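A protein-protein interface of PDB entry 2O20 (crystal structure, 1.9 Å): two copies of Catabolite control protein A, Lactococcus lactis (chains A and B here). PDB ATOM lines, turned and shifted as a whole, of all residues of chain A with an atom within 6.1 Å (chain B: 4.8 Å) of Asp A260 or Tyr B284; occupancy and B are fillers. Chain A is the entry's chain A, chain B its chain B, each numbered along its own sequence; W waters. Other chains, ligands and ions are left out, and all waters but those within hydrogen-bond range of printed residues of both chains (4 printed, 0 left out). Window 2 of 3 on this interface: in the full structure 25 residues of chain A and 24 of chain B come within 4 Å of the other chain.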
ATOM      1  N   LYS A 229     -21.881  24.274  -8.048  1.00  0.00           N
ATOM      2  CA  LYS A 229     -22.424  22.980  -8.418  1.00  0.00           C
ATOM      3  C   LYS A 229     -23.034  23.012  -9.816  1.00  0.00           C
ATOM      4  O   LYS A 229     -22.792  22.111 -10.598  1.00  0.00           O
ATOM      5  CB  LYS A 229     -23.445  22.491  -7.377  1.00  0.00           C
ATOM      6  CG  LYS A 229     -22.827  21.729  -6.192  1.00  0.00           C
ATOM      7  CD  LYS A 229     -23.891  20.982  -5.398  1.00  0.00           C
ATOM      8  CE  LYS A 229     -23.293  19.930  -4.476  1.00  0.00           C
ATOM      9  NZ  LYS A 229     -23.057  18.544  -5.087  1.00  0.00           N
ATOM     10  N   VAL A 252     -15.811  24.792  -3.678  1.00  0.00           N
ATOM     11  CA  VAL A 252     -16.359  23.601  -2.980  1.00  0.00           C
ATOM     12  C   VAL A 252     -17.575  23.005  -3.719  1.00  0.00           C
ATOM     13  O   VAL A 252     -17.651  21.787  -3.915  1.00  0.00           O
ATOM     14  CB  VAL A 252     -16.696  23.896  -1.513  1.00  0.00           C
ATOM     15  CG1 VAL A 252     -17.473  22.747  -0.864  1.00  0.00           C
ATOM     16  CG2 VAL A 252     -15.395  24.211  -0.717  1.00  0.00           C
ATOM     17  N   LEU A 255     -16.280  21.310  -7.090  1.00  0.00           N
ATOM     18  CA  LEU A 255     -15.591  20.046  -6.819  1.00  0.00           C
ATOM     19  C   LEU A 255     -16.586  18.947  -6.471  1.00  0.00           C
ATOM     20  O   LEU A 255     -16.450  17.815  -6.931  1.00  0.00           O
ATOM     21  CB  LEU A 255     -14.603  20.208  -5.677  1.00  0.00           C
ATOM     22  CG  LEU A 255     -13.863  18.945  -5.217  1.00  0.00           C
ATOM     23  CD1 LEU A 255     -13.038  18.293  -6.327  1.00  0.00           C
ATOM     24  CD2 LEU A 255     -13.004  19.285  -4.025  1.00  0.00           C
ATOM     25  N   SER A 256     -17.559  19.311  -5.649  1.00  0.00           N
ATOM     26  CA  SER A 256     -18.587  18.382  -5.196  1.00  0.00           C
ATOM     27  C   SER A 256     -19.390  17.839  -6.391  1.00  0.00           C
ATOM     28  O   SER A 256     -19.624  16.622  -6.488  1.00  0.00           O
ATOM     29  CB  SER A 256     -19.463  19.073  -4.141  1.00  0.00           C
ATOM     30  OG  SER A 256     -18.676  19.445  -2.977  1.00  0.00           O
ATOM     31  N   ALA A 257     -19.791  18.724  -7.308  1.00  0.00           N
ATOM     32  CA  ALA A 257     -20.502  18.309  -8.525  1.00  0.00           C
ATOM     33  C   ALA A 257     -19.632  17.422  -9.448  1.00  0.00           C
ATOM     34  O   ALA A 257     -20.134  16.442 -10.021  1.00  0.00           O
ATOM     35  CB  ALA A 257     -21.018  19.520  -9.274  1.00  0.00           C
ATOM     36  N   MET A 258     -18.355  17.758  -9.606  1.00  0.00           N
ATOM     37  CA  MET A 258     -17.422  16.941 -10.426  1.00  0.00           C
ATOM     38  C   MET A 258     -17.292  15.526  -9.850  1.00  0.00           C
ATOM     39  O   MET A 258     -17.357  14.519 -10.582  1.00  0.00           O
ATOM     40  CB  MET A 258     -16.028  17.584 -10.512  1.00  0.00           C
ATOM     41  CG  MET A 258     -15.942  18.886 -11.351  1.00  0.00           C
ATOM     42  SD  MET A 258     -16.388  18.592 -13.079  1.00  0.00           S
ATOM     43  CE  MET A 258     -16.257  20.230 -13.814  1.00  0.00           C
ATOM     44  N   MET A 259     -17.134  15.462  -8.534  1.00  0.00           N
ATOM     45  CA  MET A 259     -16.966  14.191  -7.850  1.00  0.00           C
ATOM     46  C   MET A 259     -18.238  13.348  -7.993  1.00  0.00           C
ATOM     47  O   MET A 259     -18.157  12.153  -8.285  1.00  0.00           O
ATOM     48  CB  MET A 259     -16.584  14.417  -6.381  1.00  0.00           C
ATOM     49  CG  MET A 259     -15.151  14.941  -6.187  1.00  0.00           C
ATOM     50  SD  MET A 259     -13.857  13.909  -6.845  1.00  0.00           S
ATOM     51  CE  MET A 259     -13.885  12.548  -5.670  1.00  0.00           C
ATOM     52  N   ASP A 260     -19.403  13.969  -7.817  1.00  0.00           N
ATOM     53  CA  ASP A 260     -20.684  13.254  -7.957  1.00  0.00           C
ATOM     54  C   ASP A 260     -20.987  12.793  -9.396  1.00  0.00           C
ATOM     55  O   ASP A 260     -21.787  11.866  -9.581  1.00  0.00           O
ATOM     56  CB  ASP A 260     -21.852  14.119  -7.460  1.00  0.00           C
ATOM     57  CG  ASP A 260     -22.007  14.126  -5.937  1.00  0.00           C
ATOM     58  OD1 ASP A 260     -21.429  13.266  -5.219  1.00  0.00           O
ATOM     59  OD2 ASP A 260     -22.750  15.006  -5.462  1.00  0.00           O
ATOM     60  N   LYS A 261     -20.393  13.454 -10.395  1.00  0.00           N
ATOM     61  CA  LYS A 261     -20.448  13.026 -11.804  1.00  0.00           C
ATOM     62  C   LYS A 261     -19.413  11.930 -12.123  1.00  0.00           C
ATOM     63  O   LYS A 261     -19.421  11.364 -13.214  1.00  0.00           O
ATOM     64  CB  LYS A 261     -20.235  14.216 -12.752  1.00  0.00           C
ATOM     65  CG  LYS A 261     -21.361  15.248 -12.713  1.00  0.00           C
ATOM     66  CD  LYS A 261     -21.037  16.524 -13.476  1.00  0.00           C
ATOM     67  CE  LYS A 261     -22.307  17.285 -13.847  1.00  0.00           C
ATOM     68  NZ  LYS A 261     -23.116  17.669 -12.658  1.00  0.00           N
ATOM     69  N   GLY A 262     -18.530  11.629 -11.176  1.00  0.00           N
ATOM     70  CA  GLY A 262     -17.504  10.617 -11.371  1.00  0.00           C
ATOM     71  C   GLY A 262     -16.302  11.091 -12.171  1.00  0.00           C
ATOM     72  O   GLY A 262     -15.514  10.280 -12.676  1.00  0.00           O
ATOM     73  N   VAL A 263     -16.128  12.404 -12.263  1.00  0.00           N
ATOM     74  CA  VAL A 263     -14.932  12.981 -12.874  1.00  0.00           C
ATOM     75  C   VAL A 263     -13.738  12.754 -11.953  1.00  0.00           C
ATOM     76  O   VAL A 263     -13.836  12.949 -10.736  1.00  0.00           O
ATOM     77  CB  VAL A 263     -15.149  14.482 -13.167  1.00  0.00           C
ATOM     78  CG1 VAL A 263     -13.876  15.141 -13.625  1.00  0.00           C
ATOM     79  CG2 VAL A 263     -16.269  14.651 -14.229  1.00  0.00           C
ATOM     80  N   TYR A 282     -12.148  21.087   3.808  1.00  0.00           N
ATOM     81  CA  TYR A 282     -13.251  20.237   4.277  1.00  0.00           C
ATOM     82  C   TYR A 282     -13.791  19.266   3.203  1.00  0.00           C
ATOM     83  O   TYR A 282     -14.601  18.382   3.512  1.00  0.00           O
ATOM     84  CB  TYR A 282     -14.405  21.110   4.791  1.00  0.00           C
ATOM     85  CG  TYR A 282     -14.100  21.970   5.993  1.00  0.00           C
ATOM     86  CD1 TYR A 282     -12.905  21.849   6.710  1.00  0.00           C
ATOM     87  CD2 TYR A 282     -15.051  22.877   6.463  1.00  0.00           C
ATOM     88  CE1 TYR A 282     -12.650  22.642   7.836  1.00  0.00           C
ATOM     89  CE2 TYR A 282     -14.790  23.686   7.571  1.00  0.00           C
ATOM     90  CZ  TYR A 282     -13.606  23.566   8.257  1.00  0.00           C
ATOM     91  OH  TYR A 282     -13.333  24.359   9.359  1.00  0.00           O
ATOM     92  N   THR A 283     -13.322  19.433   1.975  1.00  0.00           N
ATOM     93  CA  THR A 283     -13.573  18.491   0.876  1.00  0.00           C
ATOM     94  C   THR A 283     -12.442  17.490   0.740  1.00  0.00           C
ATOM     95  O   THR A 283     -11.309  17.809   1.072  1.00  0.00           O
ATOM     96  CB  THR A 283     -13.728  19.185  -0.484  1.00  0.00           C
ATOM     97  OG1 THR A 283     -12.530  19.885  -0.824  1.00  0.00           O
ATOM     98  CG2 THR A 283     -14.897  20.131  -0.491  1.00  0.00           C
ATOM     99  N   TYR A 284     -12.772  16.287   0.267  1.00  0.00           N
ATOM    100  CA  TYR A 284     -11.781  15.356  -0.278  1.00  0.00           C
ATOM    101  C   TYR A 284     -12.164  14.968  -1.706  1.00  0.00           C
ATOM    102  O   TYR A 284     -13.216  14.350  -1.924  1.00  0.00           O
ATOM    103  CB  TYR A 284     -11.538  14.110   0.604  1.00  0.00           C
ATOM    104  CG  TYR A 284     -10.231  13.417   0.219  1.00  0.00           C
ATOM    105  CD1 TYR A 284      -9.006  13.763   0.826  1.00  0.00           C
ATOM    106  CD2 TYR A 284     -10.198  12.513  -0.838  1.00  0.00           C
ATOM    107  CE1 TYR A 284      -7.785  13.137   0.436  1.00  0.00           C
ATOM    108  CE2 TYR A 284      -9.001  11.919  -1.252  1.00  0.00           C
ATOM    109  CZ  TYR A 284      -7.809  12.235  -0.636  1.00  0.00           C
ATOM    110  OH  TYR A 284      -6.660  11.602  -1.075  1.00  0.00           O
ATOM    111  N   PRO A 285     -11.286  15.255  -2.682  1.00  0.00           N
ATOM    112  CA  PRO A 285      -9.956  15.894  -2.534  1.00  0.00           C
ATOM    113  C   PRO A 285      -9.980  17.293  -1.932  1.00  0.00           C
ATOM    114  O   PRO A 285     -10.901  18.083  -2.228  1.00  0.00           O
ATOM    115  CB  PRO A 285      -9.435  15.994  -3.978  1.00  0.00           C
ATOM    116  CG  PRO A 285     -10.588  15.614  -4.855  1.00  0.00           C
ATOM    117  CD  PRO A 285     -11.547  14.839  -4.073  1.00  0.00           C
ATOM    118  N   MET B 259     -10.870  10.279   5.044  1.00  0.00           N
ATOM    119  CA  MET B 259     -10.697  10.401   3.592  1.00  0.00           C
ATOM    120  C   MET B 259      -9.213  10.503   3.134  1.00  0.00           C
ATOM    121  O   MET B 259      -8.829   9.894   2.136  1.00  0.00           O
ATOM    122  CB  MET B 259     -11.511  11.567   3.028  1.00  0.00           C
ATOM    123  CG  MET B 259     -13.011  11.542   3.298  1.00  0.00           C
ATOM    124  SD  MET B 259     -13.829  10.028   2.638  1.00  0.00           S
ATOM    125  CE  MET B 259     -13.563  10.217   0.910  1.00  0.00           C
ATOM    126  N   TYR B 282     -20.278  22.436   3.473  1.00  0.00           N
ATOM    127  CA  TYR B 282     -19.118  22.482   2.600  1.00  0.00           C
ATOM    128  C   TYR B 282     -18.263  21.215   2.706  1.00  0.00           C
ATOM    129  O   TYR B 282     -17.166  21.162   2.188  1.00  0.00           O
ATOM    130  CB  TYR B 282     -18.299  23.744   2.908  1.00  0.00           C
ATOM    131  CG  TYR B 282     -19.094  25.008   2.642  1.00  0.00           C
ATOM    132  CD1 TYR B 282     -19.364  25.408   1.345  1.00  0.00           C
ATOM    133  CD2 TYR B 282     -19.612  25.762   3.693  1.00  0.00           C
ATOM    134  CE1 TYR B 282     -20.094  26.549   1.088  1.00  0.00           C
ATOM    135  CE2 TYR B 282     -20.359  26.897   3.463  1.00  0.00           C
ATOM    136  CZ  TYR B 282     -20.607  27.281   2.152  1.00  0.00           C
ATOM    137  OH  TYR B 282     -21.353  28.385   1.912  1.00  0.00           O
ATOM    138  N   THR B 283     -18.757  20.177   3.362  1.00  0.00           N
ATOM    139  CA  THR B 283     -17.997  18.931   3.395  1.00  0.00           C
ATOM    140  C   THR B 283     -18.204  18.119   2.107  1.00  0.00           C
ATOM    141  O   THR B 283     -19.270  18.134   1.495  1.00  0.00           O
ATOM    142  CB  THR B 283     -18.311  18.076   4.625  1.00  0.00           C
ATOM    143  OG1 THR B 283     -19.638  17.545   4.517  1.00  0.00           O
ATOM    144  CG2 THR B 283     -18.173  18.913   5.884  1.00  0.00           C
ATOM    145  N   TYR B 284     -17.177  17.381   1.725  1.00  0.00           N
ATOM    146  CA  TYR B 284     -17.308  16.306   0.736  1.00  0.00           C
ATOM    147  C   TYR B 284     -16.456  15.137   1.177  1.00  0.00           C
ATOM    148  O   TYR B 284     -15.260  15.301   1.396  1.00  0.00           O
ATOM    149  CB  TYR B 284     -16.918  16.734  -0.676  1.00  0.00           C
ATOM    150  CG  TYR B 284     -17.430  15.730  -1.710  1.00  0.00           C
ATOM    151  CD1 TYR B 284     -18.687  15.859  -2.269  1.00  0.00           C
ATOM    152  CD2 TYR B 284     -16.667  14.617  -2.063  1.00  0.00           C
ATOM    153  CE1 TYR B 284     -19.171  14.908  -3.196  1.00  0.00           C
ATOM    154  CE2 TYR B 284     -17.134  13.672  -2.971  1.00  0.00           C
ATOM    155  CZ  TYR B 284     -18.387  13.816  -3.530  1.00  0.00           C
ATOM    156  OH  TYR B 284     -18.824  12.883  -4.440  1.00  0.00           O
ATOM    157  N   PRO B 285     -17.068  13.955   1.355  1.00  0.00           N
ATOM    158  CA  PRO B 285     -18.512  13.635   1.278  1.00  0.00           C
ATOM    159  C   PRO B 285     -19.402  14.431   2.230  1.00  0.00           C
ATOM    160  O   PRO B 285     -18.929  14.985   3.234  1.00  0.00           O
ATOM    161  CB  PRO B 285     -18.575  12.135   1.660  1.00  0.00           C
ATOM    162  CG  PRO B 285     -17.337  11.803   2.185  1.00  0.00           C
ATOM    163  CD  PRO B 285     -16.289  12.742   1.623  1.00  0.00           C
ATOM    164  N   THR B 286     -20.682  14.473   1.903  1.00  0.00           N
ATOM    165  CA  THR B 286     -21.659  15.154   2.732  1.00  0.00           C
ATOM    166  C   THR B 286     -21.816  14.487   4.099  1.00  0.00           C
ATOM    167  O   THR B 286     -21.698  13.262   4.245  1.00  0.00           O
ATOM    168  CB  THR B 286     -23.037  15.311   2.030  1.00  0.00           C
ATOM    169  OG1 THR B 286     -23.605  14.028   1.768  1.00  0.00           O
ATOM    170  CG2 THR B 286     -22.910  16.092   0.765  1.00  0.00           C
ATOM    171  N   ARG B 329     -24.186  11.529   3.218  1.00  0.00           N
ATOM    172  CA  ARG B 329     -23.355  10.451   2.680  1.00  0.00           C
ATOM    173  C   ARG B 329     -22.221   9.970   3.614  1.00  0.00           C
ATOM    174  O   ARG B 329     -21.417   9.137   3.201  1.00  0.00           O
ATOM    175  CB  ARG B 329     -22.838  10.840   1.297  1.00  0.00           C
ATOM    176  CG  ARG B 329     -24.024  11.078   0.331  1.00  0.00           C
ATOM    177  CD  ARG B 329     -23.646  11.070  -1.119  1.00  0.00           C
ATOM    178  NE  ARG B 329     -24.802  11.217  -2.018  1.00  0.00           N
ATOM    179  CZ  ARG B 329     -25.442  12.361  -2.303  1.00  0.00           C
ATOM    180  NH1 ARG B 329     -25.101  13.532  -1.750  1.00  0.00           N
ATOM    181  NH2 ARG B 329     -26.457  12.333  -3.160  1.00  0.00           N
HETATM  182  O   HOH W   1     -20.548  18.973  -0.865  1.00  0.00           O
HETATM  183  O   HOH W   2     -22.749  11.411  -3.953  1.00  0.00           O
HETATM  184  O   HOH W   3     -13.419  15.120   3.655  1.00  0.00           O
HETATM  185  O   HOH W   4     -22.748  14.742  -2.401  1.00  0.00           O
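O of Tyr A282 lies within hydrogen-bond range of N of Tyr B284. The side-chain carboxylate (OD1) of Asp A260 sits at hydrogen-bond distance from the side-chain hydroxyl (OH) of Tyr B284 (2.7 Å). The backbone NH of Tyr A284 lies within hydrogen-bond range of the backbone carbonyl oxygen of Tyr B284 (2.9 Å).
Tyr A282 touches its own counterpart, Tyr B282. Tyr A282 touches Thr B283, and with the chains exchanged Thr A283 touches Tyr B282. Tyr A282 touches Tyr B284, but with the chains exchanged Tyr A284 does not touch Tyr B282 (6.8 Å). Tyr A284 touches its own counterpart, Tyr B284. Of the 11 pairs that touch across the chains among the printed residues, 6 have their exchanged pair printed and touching as well.
Water W2 lies within hydrogen-bond range of the side-chain carboxylate (OD1) of Asp A260 and the guanidinium group (NE) of Arg B329. Water W4 bridges NH1 of Arg B329 and OD2 of Asp A260. Water W1 lies within hydrogen-bond range of O of Thr B283 and OG of Ser A256. Water W3 bridges the backbone carbonyl oxygen of Tyr B284 (2.9 Å) and the backbone carbonyl oxygen of Tyr A282 (3.5 Å).
O of Tyr B282 touches CG1 of Val A252 (3.5 Å). Ser A256 touches Tyr B284. Met A259 touches Tyr B284. CB of Tyr A282 touches O of Tyr B282, at 3.8 Å. Tyr A282 touches Thr B283. Thr A283 touches Tyr B282 (CG2 to O, 3.7 Å). Tyr B284 touches Thr A283 (O to C, 3.6 Å). CB of Tyr A284 touches CB of Met B259 (3.5 Å).
Printed residues of chain B that touch a printed residue of chain A: Met B259, Tyr B282, Thr B283 and Tyr B284. Hydrophobic or aromatic side chains of chain B within 4 Å of the printed part of chain A: Met B259, Tyr B282 and Tyr B284. Printed residues of chain A that touch a printed residue of chain B: Val A252, Ser A256, Met A259, Asp A260, Tyr A282, Thr A283 and Tyr A284. Among the printed residues, 11 pairs touch across the chains.
Of the printed residues of chain B, Val A252 touches Tyr B282. Printed residues of chain B within 4 Å of Ser A256: Tyr B284 (3.7 Å). Of chain B, only Tyr B284 comes within 4 Å of Asp A260. Of the printed residues of chain A, Tyr B282 touches Val A252, Tyr A282 and Thr A283. Of chain A, only Ser A256 (3.7 Å), Met A259 (3.3 Å), Asp A260 (2.7 Å), Tyr A282 (3.3 Å), Thr A283 (3.6 Å) and Tyr A284 (2.9 Å) come within 4 Å of Tyr B284.
The backbone carbonyl oxygen of Pro A285 is in hydrogen-bond range of the side-chain hydroxyl of Thr A283. The side-chain hydroxyl of Thr B283 sits at hydrogen-bond distance from the backbone carbonyl oxygen of Pro B285. The backbone carbonyl oxygen of Val A252 is in hydrogen-bond range of the side-chain hydroxyl of Ser A256 (2.7 Å). NZ of Lys A229 lies within salt-bridge range of OD2 of Asp A260 (3.6 Å).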
